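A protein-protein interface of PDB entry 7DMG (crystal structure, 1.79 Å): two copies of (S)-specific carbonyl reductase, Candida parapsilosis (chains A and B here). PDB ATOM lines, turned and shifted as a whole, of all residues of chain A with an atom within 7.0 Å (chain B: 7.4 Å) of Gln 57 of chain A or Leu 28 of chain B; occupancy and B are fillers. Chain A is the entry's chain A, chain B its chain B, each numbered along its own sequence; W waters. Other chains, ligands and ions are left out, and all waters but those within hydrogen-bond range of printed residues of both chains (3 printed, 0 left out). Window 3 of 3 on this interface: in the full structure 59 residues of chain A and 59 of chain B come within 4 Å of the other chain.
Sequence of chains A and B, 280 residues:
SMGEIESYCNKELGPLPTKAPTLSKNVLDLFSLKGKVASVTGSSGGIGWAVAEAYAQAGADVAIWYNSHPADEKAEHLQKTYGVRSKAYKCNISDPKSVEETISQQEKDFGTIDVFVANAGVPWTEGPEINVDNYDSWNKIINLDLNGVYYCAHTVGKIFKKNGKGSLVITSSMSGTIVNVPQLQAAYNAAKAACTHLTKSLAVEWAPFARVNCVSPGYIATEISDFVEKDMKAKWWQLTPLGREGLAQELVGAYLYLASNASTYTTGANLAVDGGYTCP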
ATOM      1  N   LEU A  28      26.444 -11.706  26.437  1.00  0.00           N
ATOM      2  CA  LEU A  28      26.851 -13.100  26.299  1.00  0.00           C
ATOM      3  C   LEU A  28      25.878 -14.044  26.999  1.00  0.00           C
ATOM      4  O   LEU A  28      25.684 -15.176  26.538  1.00  0.00           O
ATOM      5  CB  LEU A  28      28.269 -13.291  26.831  1.00  0.00           C
ATOM      6  CG  LEU A  28      29.370 -12.511  26.111  1.00  0.00           C
ATOM      7  CD1 LEU A  28      30.706 -12.694  26.815  1.00  0.00           C
ATOM      8  CD2 LEU A  28      29.455 -12.937  24.650  1.00  0.00           C
ATOM      9  N   PHE A  31      22.801 -15.635  24.894  1.00  0.00           N
ATOM     10  CA  PHE A  31      22.991 -16.766  23.998  1.00  0.00           C
ATOM     11  C   PHE A  31      22.967 -18.103  24.725  1.00  0.00           C
ATOM     12  O   PHE A  31      23.082 -19.147  24.077  1.00  0.00           O
ATOM     13  CB  PHE A  31      24.322 -16.617  23.242  1.00  0.00           C
ATOM     14  CG  PHE A  31      24.304 -15.528  22.208  1.00  0.00           C
ATOM     15  CD1 PHE A  31      24.603 -14.216  22.560  1.00  0.00           C
ATOM     16  CD2 PHE A  31      23.973 -15.808  20.895  1.00  0.00           C
ATOM     17  CE1 PHE A  31      24.564 -13.192  21.606  1.00  0.00           C
ATOM     18  CE2 PHE A  31      23.945 -14.810  19.932  1.00  0.00           C
ATOM     19  CZ  PHE A  31      24.246 -13.496  20.283  1.00  0.00           C
ATOM     20  N   SER A  32      22.822 -18.100  26.046  1.00  0.00           N
ATOM     21  CA  SER A  32      22.846 -19.349  26.797  1.00  0.00           C
ATOM     22  C   SER A  32      21.558 -20.134  26.577  1.00  0.00           C
ATOM     23  O   SER A  32      20.463 -19.565  26.512  1.00  0.00           O
ATOM     24  CB  SER A  32      23.034 -19.069  28.288  1.00  0.00           C
ATOM     25  OG  SER A  32      22.839 -20.249  29.055  1.00  0.00           O
ATOM     26  N   LEU A  33      21.694 -21.458  26.476  1.00  0.00           N
ATOM     27  CA  LEU A  33      20.552 -22.360  26.428  1.00  0.00           C
ATOM     28  C   LEU A  33      20.456 -23.236  27.672  1.00  0.00           C
ATOM     29  O   LEU A  33      19.764 -24.257  27.647  1.00  0.00           O
ATOM     30  CB  LEU A  33      20.606 -23.235  25.176  1.00  0.00           C
ATOM     31  CG  LEU A  33      20.438 -22.559  23.813  1.00  0.00           C
ATOM     32  CD1 LEU A  33      20.567 -23.600  22.688  1.00  0.00           C
ATOM     33  CD2 LEU A  33      19.117 -21.829  23.716  1.00  0.00           C
ATOM     34  N   LYS A  34      21.131 -22.852  28.759  1.00  0.00           N
ATOM     35  CA  LYS A  34      21.051 -23.609  30.006  1.00  0.00           C
ATOM     36  C   LYS A  34      19.615 -23.689  30.501  1.00  0.00           C
ATOM     37  O   LYS A  34      18.875 -22.701  30.480  1.00  0.00           O
ATOM     38  CB  LYS A  34      21.932 -22.970  31.081  1.00  0.00           C
ATOM     39  CG  LYS A  34      23.398 -22.857  30.692  1.00  0.00           C
ATOM     40  CD  LYS A  34      24.235 -22.277  31.829  1.00  0.00           C
ATOM     41  CE  LYS A  34      25.623 -22.912  31.859  1.00  0.00           C
ATOM     42  NZ  LYS A  34      26.575 -22.163  32.725  1.00  0.00           N
ATOM     43  N   ALA A  50      26.204 -30.511  13.700  1.00  0.00           N
ATOM     44  CA  ALA A  50      26.912 -29.302  14.119  1.00  0.00           C
ATOM     45  C   ALA A  50      26.041 -28.441  15.023  1.00  0.00           C
ATOM     46  O   ALA A  50      26.518 -27.895  16.026  1.00  0.00           O
ATOM     47  CB  ALA A  50      27.354 -28.489  12.903  1.00  0.00           C
ATOM     48  N   VAL A  51      24.766 -28.286  14.663  1.00  0.00           N
ATOM     49  CA  VAL A  51      23.860 -27.454  15.452  1.00  0.00           C
ATOM     50  C   VAL A  51      23.567 -28.110  16.802  1.00  0.00           C
ATOM     51  O   VAL A  51      23.534 -27.439  17.843  1.00  0.00           O
ATOM     52  CB  VAL A  51      22.567 -27.193  14.655  1.00  0.00           C
ATOM     53  CG1 VAL A  51      21.454 -26.677  15.571  1.00  0.00           C
ATOM     54  CG2 VAL A  51      22.824 -26.228  13.508  1.00  0.00           C
ATOM     55  N   ALA A  52      23.363 -29.429  16.807  1.00  0.00           N
ATOM     56  CA  ALA A  52      23.108 -30.146  18.055  1.00  0.00           C
ATOM     57  C   ALA A  52      24.264 -29.994  19.033  1.00  0.00           C
ATOM     58  O   ALA A  52      24.055 -29.713  20.218  1.00  0.00           O
ATOM     59  CB  ALA A  52      22.853 -31.626  17.764  1.00  0.00           C
ATOM     60  N   GLU A  53      25.502 -30.209  18.564  1.00  0.00           N
ATOM     61  CA  GLU A  53      26.640 -30.069  19.468  1.00  0.00           C
ATOM     62  C   GLU A  53      26.796 -28.623  19.935  1.00  0.00           C
ATOM     63  O   GLU A  53      27.144 -28.374  21.095  1.00  0.00           O
ATOM     64  CB  GLU A  53      27.925 -30.573  18.812  1.00  0.00           C
ATOM     65  CG  GLU A  53      29.109 -30.533  19.783  1.00  0.00           C
ATOM     66  CD  GLU A  53      30.292 -31.379  19.350  1.00  0.00           C
ATOM     67  OE1 GLU A  53      30.262 -31.948  18.237  1.00  0.00           O
ATOM     68  OE2 GLU A  53      31.248 -31.483  20.143  1.00  0.00           O
ATOM     69  N   ALA A  54      26.510 -27.655  19.059  1.00  0.00           N
ATOM     70  CA  ALA A  54      26.558 -26.258  19.480  1.00  0.00           C
ATOM     71  C   ALA A  54      25.538 -25.981  20.578  1.00  0.00           C
ATOM     72  O   ALA A  54      25.835 -25.278  21.554  1.00  0.00           O
ATOM     73  CB  ALA A  54      26.312 -25.333  18.290  1.00  0.00           C
ATOM     74  N   TYR A  55      24.328 -26.520  20.432  1.00  0.00           N
ATOM     75  CA  TYR A  55      23.304 -26.301  21.448  1.00  0.00           C
ATOM     76  C   TYR A  55      23.724 -26.918  22.774  1.00  0.00           C
ATOM     77  O   TYR A  55      23.506 -26.327  23.839  1.00  0.00           O
ATOM     78  CB  TYR A  55      21.964 -26.875  20.973  1.00  0.00           C
ATOM     79  CG  TYR A  55      21.236 -26.030  19.935  1.00  0.00           C
ATOM     80  CD1 TYR A  55      21.766 -24.825  19.473  1.00  0.00           C
ATOM     81  CD2 TYR A  55      20.017 -26.443  19.424  1.00  0.00           C
ATOM     82  CE1 TYR A  55      21.095 -24.056  18.517  1.00  0.00           C
ATOM     83  CE2 TYR A  55      19.329 -25.682  18.487  1.00  0.00           C
ATOM     84  CZ  TYR A  55      19.864 -24.493  18.034  1.00  0.00           C
ATOM     85  OH  TYR A  55      19.165 -23.761  17.092  1.00  0.00           O
ATOM     86  N   ALA A  56      24.351 -28.103  22.724  1.00  0.00           N
ATOM     87  CA  ALA A  56      24.844 -28.741  23.942  1.00  0.00           C
ATOM     88  C   ALA A  56      25.937 -27.907  24.601  1.00  0.00           C
ATOM     89  O   ALA A  56      25.984 -27.799  25.832  1.00  0.00           O
ATOM     90  CB  ALA A  56      25.358 -30.152  23.644  1.00  0.00           C
ATOM     91  N   GLN A  57      26.832 -27.319  23.798  1.00  0.00           N
ATOM     92  CA  GLN A  57      27.842 -26.413  24.342  1.00  0.00           C
ATOM     93  C   GLN A  57      27.209 -25.201  25.017  1.00  0.00           C
ATOM     94  O   GLN A  57      27.763 -24.670  25.989  1.00  0.00           O
ATOM     95  CB  GLN A  57      28.787 -25.963  23.227  1.00  0.00           C
ATOM     96  CG  GLN A  57      29.704 -27.067  22.734  1.00  0.00           C
ATOM     97  CD  GLN A  57      30.410 -26.694  21.454  1.00  0.00           C
ATOM     98  OE1 GLN A  57      30.048 -25.718  20.794  1.00  0.00           O
ATOM     99  NE2 GLN A  57      31.421 -27.468  21.093  1.00  0.00           N
ATOM    100  N   ALA A  58      26.055 -24.752  24.524  1.00  0.00           N
ATOM    101  CA  ALA A  58      25.327 -23.645  25.131  1.00  0.00           C
ATOM    102  C   ALA A  58      24.511 -24.072  26.344  1.00  0.00           C
ATOM    103  O   ALA A  58      23.869 -23.218  26.973  1.00  0.00           O
ATOM    104  CB  ALA A  58      24.416 -22.984  24.092  1.00  0.00           C
ATOM    105  N   GLY A  59      24.513 -25.357  26.684  1.00  0.00           N
ATOM    106  CA  GLY A  59      23.883 -25.834  27.894  1.00  0.00           C
ATOM    107  C   GLY A  59      22.554 -26.533  27.723  1.00  0.00           C
ATOM    108  O   GLY A  59      21.933 -26.883  28.731  1.00  0.00           O
ATOM    109  N   ALA A  60      22.099 -26.755  26.493  1.00  0.00           N
ATOM    110  CA  ALA A  60      20.792 -27.355  26.277  1.00  0.00           C
ATOM    111  C   ALA A  60      20.859 -28.877  26.319  1.00  0.00           C
ATOM    112  O   ALA A  60      21.846 -29.486  25.899  1.00  0.00           O
ATOM    113  CB  ALA A  60      20.206 -26.920  24.936  1.00  0.00           C
ATOM    114  N   VAL A  62      19.549 -32.060  24.395  1.00  0.00           N
ATOM    115  CA  VAL A  62      19.398 -32.169  22.945  1.00  0.00           C
ATOM    116  C   VAL A  62      18.781 -33.517  22.595  1.00  0.00           C
ATOM    117  O   VAL A  62      19.352 -34.569  22.907  1.00  0.00           O
ATOM    118  CB  VAL A  62      20.735 -31.987  22.203  1.00  0.00           C
ATOM    119  CG1 VAL A  62      20.499 -32.020  20.704  1.00  0.00           C
ATOM    120  CG2 VAL A  62      21.406 -30.671  22.605  1.00  0.00           C
ATOM    121  N   LEU A  78      27.254 -36.355  23.473  1.00  0.00           N
ATOM    122  CA  LEU A  78      26.855 -35.074  24.062  1.00  0.00           C
ATOM    123  C   LEU A  78      26.705 -35.175  25.582  1.00  0.00           C
ATOM    124  O   LEU A  78      27.131 -34.271  26.314  1.00  0.00           O
ATOM    125  CB  LEU A  78      25.546 -34.593  23.424  1.00  0.00           C
ATOM    126  CG  LEU A  78      25.562 -34.228  21.940  1.00  0.00           C
ATOM    127  CD1 LEU A  78      24.217 -33.653  21.525  1.00  0.00           C
ATOM    128  CD2 LEU A  78      26.695 -33.255  21.628  1.00  0.00           C
ATOM    129  N   TYR A  82      29.437 -32.908  27.619  1.00  0.00           N
ATOM    130  CA  TYR A  82      28.900 -31.650  28.098  1.00  0.00           C
ATOM    131  C   TYR A  82      27.985 -31.801  29.304  1.00  0.00           C
ATOM    132  O   TYR A  82      27.533 -30.787  29.841  1.00  0.00           O
ATOM    133  CB  TYR A  82      28.159 -30.939  26.962  1.00  0.00           C
ATOM    134  CG  TYR A  82      29.044 -30.717  25.758  1.00  0.00           C
ATOM    135  CD1 TYR A  82      30.060 -29.766  25.792  1.00  0.00           C
ATOM    136  CD2 TYR A  82      28.884 -31.468  24.596  1.00  0.00           C
ATOM    137  CE1 TYR A  82      30.886 -29.568  24.701  1.00  0.00           C
ATOM    138  CE2 TYR A  82      29.712 -31.270  23.493  1.00  0.00           C
ATOM    139  CZ  TYR A  82      30.706 -30.320  23.557  1.00  0.00           C
ATOM    140  OH  TYR A  82      31.523 -30.108  22.476  1.00  0.00           O
ATOM    141  N   VAL A  84      24.938 -32.766  29.518  1.00  0.00           N
ATOM    142  CA  VAL A  84      23.525 -32.515  29.271  1.00  0.00           C
ATOM    143  C   VAL A  84      22.821 -33.845  29.025  1.00  0.00           C
ATOM    144  O   VAL A  84      23.453 -34.878  28.787  1.00  0.00           O
ATOM    145  CB  VAL A  84      23.325 -31.552  28.083  1.00  0.00           C
ATOM    146  CG1 VAL A  84      23.910 -30.191  28.411  1.00  0.00           C
ATOM    147  CG2 VAL A  84      23.951 -32.128  26.817  1.00  0.00           C
ATOM    148  N   GLN A 249      30.430 -25.415  10.778  1.00  0.00           N
ATOM    149  CA  GLN A 249      30.692 -24.613  11.968  1.00  0.00           C
ATOM    150  C   GLN A 249      30.395 -23.135  11.741  1.00  0.00           C
ATOM    151  O   GLN A 249      30.145 -22.408  12.707  1.00  0.00           O
ATOM    152  CB  GLN A 249      32.139 -24.830  12.434  1.00  0.00           C
ATOM    153  CG  GLN A 249      32.460 -24.203  13.794  1.00  0.00           C
ATOM    154  CD  GLN A 249      31.744 -24.881  14.959  1.00  0.00           C
ATOM    155  OE1 GLN A 249      30.979 -25.840  14.778  1.00  0.00           O
ATOM    156  NE2 GLN A 249      31.997 -24.387  16.169  1.00  0.00           N
ATOM    157  N   VAL A 252      26.548 -22.463  13.001  1.00  0.00           N
ATOM    158  CA  VAL A 252      26.003 -22.676  14.341  1.00  0.00           C
ATOM    159  C   VAL A 252      25.717 -21.357  15.055  1.00  0.00           C
ATOM    160  O   VAL A 252      24.794 -21.283  15.876  1.00  0.00           O
ATOM    161  CB  VAL A 252      26.934 -23.582  15.173  1.00  0.00           C
ATOM    162  CG1 VAL A 252      27.062 -24.974  14.531  1.00  0.00           C
ATOM    163  CG2 VAL A 252      28.309 -22.944  15.378  1.00  0.00           C
ATOM    164  N   LEU A 256      22.232 -20.632  16.989  1.00  0.00           N
ATOM    165  CA  LEU A 256      22.188 -20.303  18.414  1.00  0.00           C
ATOM    166  C   LEU A 256      21.565 -18.928  18.634  1.00  0.00           C
ATOM    167  O   LEU A 256      20.796 -18.724  19.583  1.00  0.00           O
ATOM    168  CB  LEU A 256      23.594 -20.378  19.026  1.00  0.00           C
ATOM    169  CG  LEU A 256      23.666 -20.062  20.532  1.00  0.00           C
ATOM    170  CD1 LEU A 256      22.916 -21.120  21.344  1.00  0.00           C
ATOM    171  CD2 LEU A 256      25.109 -19.908  21.034  1.00  0.00           C
ATOM    172  N   SER B  24      36.966 -21.507  16.423  1.00  0.00           N
ATOM    173  CA  SER B  24      36.905 -22.304  17.638  1.00  0.00           C
ATOM    174  C   SER B  24      35.857 -23.405  17.495  1.00  0.00           C
ATOM    175  O   SER B  24      34.854 -23.249  16.793  1.00  0.00           O
ATOM    176  CB  SER B  24      36.568 -21.431  18.848  1.00  0.00           C
ATOM    177  OG  SER B  24      36.202 -22.245  19.956  1.00  0.00           O
ATOM    178  N   LYS B  25      36.097 -24.531  18.176  1.00  0.00           N
ATOM    179  CA  LYS B  25      35.101 -25.597  18.186  1.00  0.00           C
ATOM    180  C   LYS B  25      33.962 -25.335  19.157  1.00  0.00           C
ATOM    181  O   LYS B  25      32.956 -26.051  19.107  1.00  0.00           O
ATOM    182  CB  LYS B  25      35.725 -26.943  18.545  1.00  0.00           C
ATOM    183  CG  LYS B  25      36.731 -27.479  17.562  1.00  0.00           C
ATOM    184  CD  LYS B  25      37.319 -28.750  18.148  1.00  0.00           C
ATOM    185  CE  LYS B  25      38.357 -29.353  17.264  1.00  0.00           C
ATOM    186  NZ  LYS B  25      38.011 -30.710  16.741  1.00  0.00           N
ATOM    187  N   ASN B  26      34.097 -24.356  20.044  1.00  0.00           N
ATOM    188  CA  ASN B  26      33.049 -24.026  20.999  1.00  0.00           C
ATOM    189  C   ASN B  26      32.282 -22.814  20.483  1.00  0.00           C
ATOM    190  O   ASN B  26      32.874 -21.753  20.250  1.00  0.00           O
ATOM    191  CB  ASN B  26      33.631 -23.758  22.386  1.00  0.00           C
ATOM    192  CG  ASN B  26      32.547 -23.529  23.426  1.00  0.00           C
ATOM    193  OD1 ASN B  26      31.898 -22.481  23.436  1.00  0.00           O
ATOM    194  ND2 ASN B  26      32.332 -24.515  24.295  1.00  0.00           N
ATOM    195  N   VAL B  27      30.965 -22.978  20.311  1.00  0.00           N
ATOM    196  CA  VAL B  27      30.144 -21.942  19.689  1.00  0.00           C
ATOM    197  C   VAL B  27      30.220 -20.646  20.480  1.00  0.00           C
ATOM    198  O   VAL B  27      30.142 -19.555  19.904  1.00  0.00           O
ATOM    199  CB  VAL B  27      28.682 -22.422  19.536  1.00  0.00           C
ATOM    200  CG1 VAL B  27      28.076 -22.780  20.890  1.00  0.00           C
ATOM    201  CG2 VAL B  27      27.829 -21.368  18.829  1.00  0.00           C
ATOM    202  N   LEU B  28      30.401 -20.726  21.799  1.00  0.00           N
ATOM    203  CA  LEU B  28      30.316 -19.490  22.559  1.00  0.00           C
ATOM    204  C   LEU B  28      31.558 -18.632  22.330  1.00  0.00           C
ATOM    205  O   LEU B  28      31.468 -17.398  22.328  1.00  0.00           O
ATOM    206  CB  LEU B  28      30.152 -19.773  24.052  1.00  0.00           C
ATOM    207  CG  LEU B  28      28.717 -20.202  24.391  1.00  0.00           C
ATOM    208  CD1 LEU B  28      28.630 -21.057  25.698  1.00  0.00           C
ATOM    209  CD2 LEU B  28      27.601 -19.167  24.214  1.00  0.00           C
ATOM    210  N   ASP B  29      32.717 -19.267  22.098  1.00  0.00           N
ATOM    211  CA  ASP B  29      33.932 -18.511  21.822  1.00  0.00           C
ATOM    212  C   ASP B  29      33.857 -17.754  20.501  1.00  0.00           C
ATOM    213  O   ASP B  29      34.598 -16.781  20.316  1.00  0.00           O
ATOM    214  CB  ASP B  29      35.147 -19.439  21.801  1.00  0.00           C
ATOM    215  CG  ASP B  29      35.403 -20.099  23.144  1.00  0.00           C
ATOM    216  OD1 ASP B  29      35.132 -19.464  24.185  1.00  0.00           O
ATOM    217  OD2 ASP B  29      35.909 -21.247  23.156  1.00  0.00           O
ATOM    218  N   LEU B  30      33.000 -18.190  19.573  1.00  0.00           N
ATOM    219  CA  LEU B  30      32.878 -17.497  18.292  1.00  0.00           C
ATOM    220  C   LEU B  30      32.361 -16.078  18.470  1.00  0.00           C
ATOM    221  O   LEU B  30      32.627 -15.214  17.630  1.00  0.00           O
ATOM    222  CB  LEU B  30      31.936 -18.251  17.358  1.00  0.00           C
ATOM    223  CG  LEU B  30      32.292 -19.676  16.951  1.00  0.00           C
ATOM    224  CD1 LEU B  30      31.150 -20.250  16.134  1.00  0.00           C
ATOM    225  CD2 LEU B  30      33.587 -19.690  16.144  1.00  0.00           C
ATOM    226  N   PHE B  31      31.608 -15.826  19.532  1.00  0.00           N
ATOM    227  CA  PHE B  31      30.987 -14.522  19.732  1.00  0.00           C
ATOM    228  C   PHE B  31      31.895 -13.533  20.451  1.00  0.00           C
ATOM    229  O   PHE B  31      31.507 -12.371  20.624  1.00  0.00           O
ATOM    230  CB  PHE B  31      29.673 -14.681  20.506  1.00  0.00           C
ATOM    231  CG  PHE B  31      28.568 -15.300  19.691  1.00  0.00           C
ATOM    232  CD1 PHE B  31      28.411 -16.678  19.641  1.00  0.00           C
ATOM    233  CD2 PHE B  31      27.698 -14.505  18.961  1.00  0.00           C
ATOM    234  CE1 PHE B  31      27.404 -17.254  18.888  1.00  0.00           C
ATOM    235  CE2 PHE B  31      26.684 -15.073  18.202  1.00  0.00           C
ATOM    236  CZ  PHE B  31      26.537 -16.451  18.161  1.00  0.00           C
ATOM    237  N   SER B  32      33.081 -13.959  20.875  1.00  0.00           N
ATOM    238  CA  SER B  32      33.977 -13.074  21.604  1.00  0.00           C
ATOM    239  C   SER B  32      34.549 -12.002  20.684  1.00  0.00           C
ATOM    240  O   SER B  32      34.842 -12.257  19.511  1.00  0.00           O
ATOM    241  CB  SER B  32      35.123 -13.875  22.214  1.00  0.00           C
ATOM    242  OG  SER B  32      36.085 -12.988  22.744  1.00  0.00           O
ATOM    243  N   LEU B 256      26.184  -8.349  17.630  1.00  0.00           N
ATOM    244  CA  LEU B 256      27.343  -9.144  18.042  1.00  0.00           C
ATOM    245  C   LEU B 256      27.553 -10.338  17.119  1.00  0.00           C
ATOM    246  O   LEU B 256      28.696 -10.696  16.806  1.00  0.00           O
ATOM    247  CB  LEU B 256      27.198  -9.605  19.497  1.00  0.00           C
ATOM    248  CG  LEU B 256      28.393 -10.410  20.040  1.00  0.00           C
ATOM    249  CD1 LEU B 256      29.659  -9.562  20.051  1.00  0.00           C
ATOM    250  CD2 LEU B 256      28.128 -10.948  21.440  1.00  0.00           C
ATOM    251  N   SER B 260      31.227 -10.630  15.013  1.00  0.00           N
ATOM    252  CA  SER B 260      32.147 -11.617  15.561  1.00  0.00           C
ATOM    253  C   SER B 260      32.377 -12.764  14.578  1.00  0.00           C
ATOM    254  O   SER B 260      31.803 -12.816  13.488  1.00  0.00           O
ATOM    255  CB  SER B 260      31.604 -12.143  16.889  1.00  0.00           C
ATOM    256  OG  SER B 260      30.447 -12.938  16.657  1.00  0.00           O
ATOM    257  N   ALA B 262      31.226 -15.543  14.812  1.00  0.00           N
ATOM    258  CA  ALA B 262      30.036 -16.372  14.697  1.00  0.00           C
ATOM    259  C   ALA B 262      29.473 -16.363  13.283  1.00  0.00           C
ATOM    260  O   ALA B 262      28.701 -17.260  12.939  1.00  0.00           O
ATOM    261  CB  ALA B 262      28.957 -15.895  15.687  1.00  0.00           C
HETATM  262  O   HOH W   1      30.490 -24.710  26.492  1.00  0.00           O
HETATM  263  O   HOH W   2      28.866 -19.981  13.278  1.00  0.00           O
HETATM  264  O   HOH W   3      29.871 -25.474  18.018  1.00  0.00           O
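The side-chain amide nitrogen (NE2) of Gln 57 of chain A sits at hydrogen-bond distance from the backbone carbonyl oxygen (O) of Lys 25 of chain B. OE1 of Gln 57 of chain A lies within hydrogen-bond range of N of Val 27 of chain B (2.9 Å). The side-chain amide nitrogen of Gln 249 of chain A is in hydrogen-bond range of the backbone carbonyl oxygen of Ser 24 of chain B (3.1 Å).
The side-chain amide nitrogen (NE2) of Gln 57 of chain A sits at hydrogen-bond distance from the side-chain hydroxyl (OH) of Tyr 82 of chain A, at 3.0 Å. N of Asn 26 of chain B lies within hydrogen-bond range of OG of Ser 24 of chain B (3.0 Å). OD2 of Asp 29 of chain B lies within hydrogen-bond range of OG of Ser 24 of chain B (3.4 Å). The backbone NH (N) of Leu 28 of chain B lies within hydrogen-bond range of the side-chain amide oxygen (OD1) of Asn 26 of chain B, 2.8 Å away. O of Leu 30 of chain B sits at hydrogen-bond distance from OG of Ser 260 of chain B, at 3.3 Å. The backbone carbonyl oxygen (O) of Leu 30 of chain B lies within hydrogen-bond range of the backbone NH (N) of Ala 262 of chain B, at 3.2 Å.
Among the printed residues, merely in contact across the chains: Phe 31 of chain A with Phe 31 of chain B, Ala 54 of chain A with Val 27 of chain B, Gln 57 of chain A with Asn 26 of chain B, Gln 249 of chain A with Lys 25 of chain B, Gln 57 of chain A with Leu 28 of chain B, Leu 256 of chain A with Val 27 of chain B, Val 252 of chain A with Val 27 of chain B and Val 252 of chain A with Leu 30 of chain B.
Of chain B, only Lys 25, Asn 26, Val 27 and Leu 28 come within 4 Å of Gln 57 of chain A. Leu 28 of chain B touches just one residue of chain A: Gln 57 (3.7 Å). No residue of chain B comes within 4 Å of Ala 56 of chain A. Of the printed residues of chain A, Phe 31 of chain B touches Phe 31 (3.3 Å). Printed residues of chain A within 4 Å of Leu 30 of chain B: Val 252. Of the printed residues of chain A, Lys 25 of chain B touches Gln 57 (2.9 Å) and Gln 249 (3.5 Å). Val 84 of chain A touches none of the printed residues of chain B. The nearest residue of chain A that does not touch Leu 28 of chain B is Leu 256 of chain A (4.1 Å).
Of the 12 printed residues of chain B, 7 touch a printed residue of chain A. Hydrophobic or aromatic side chains of chain A within 4 Å of the printed part of chain B: Phe 31, Ala 54, Val 252 and Leu 256. Among the printed residues, 11 pairs touch across the chains.
Phe 31 of chain A touches its own counterpart, Phe 31 of chain B. 4 positions are printed for both chains. Of the 11 pairs that touch across the chains among the printed residues, 1 has its exchanged pair printed and touching as well.
Water W2 lies within hydrogen-bond range of O of Ala 262 of chain B (2.7 Å), O of Gln 249 of chain A (2.8 Å) and N of Val 252 of chain A (3.4 Å). Water W1 lies within hydrogen-bond range of O of Gln 57 of chain A and ND2 of Asn 26 of chain B. Water W3 lies within hydrogen-bond range of the side-chain amide oxygen (OE1) of Gln 57 of chain A (2.8 Å), the side-chain amide nitrogen (NE2) of Gln 249 of chain A (3.0 Å) and the backbone carbonyl oxygen (O) of Lys 25 of chain B (3.3 Å).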
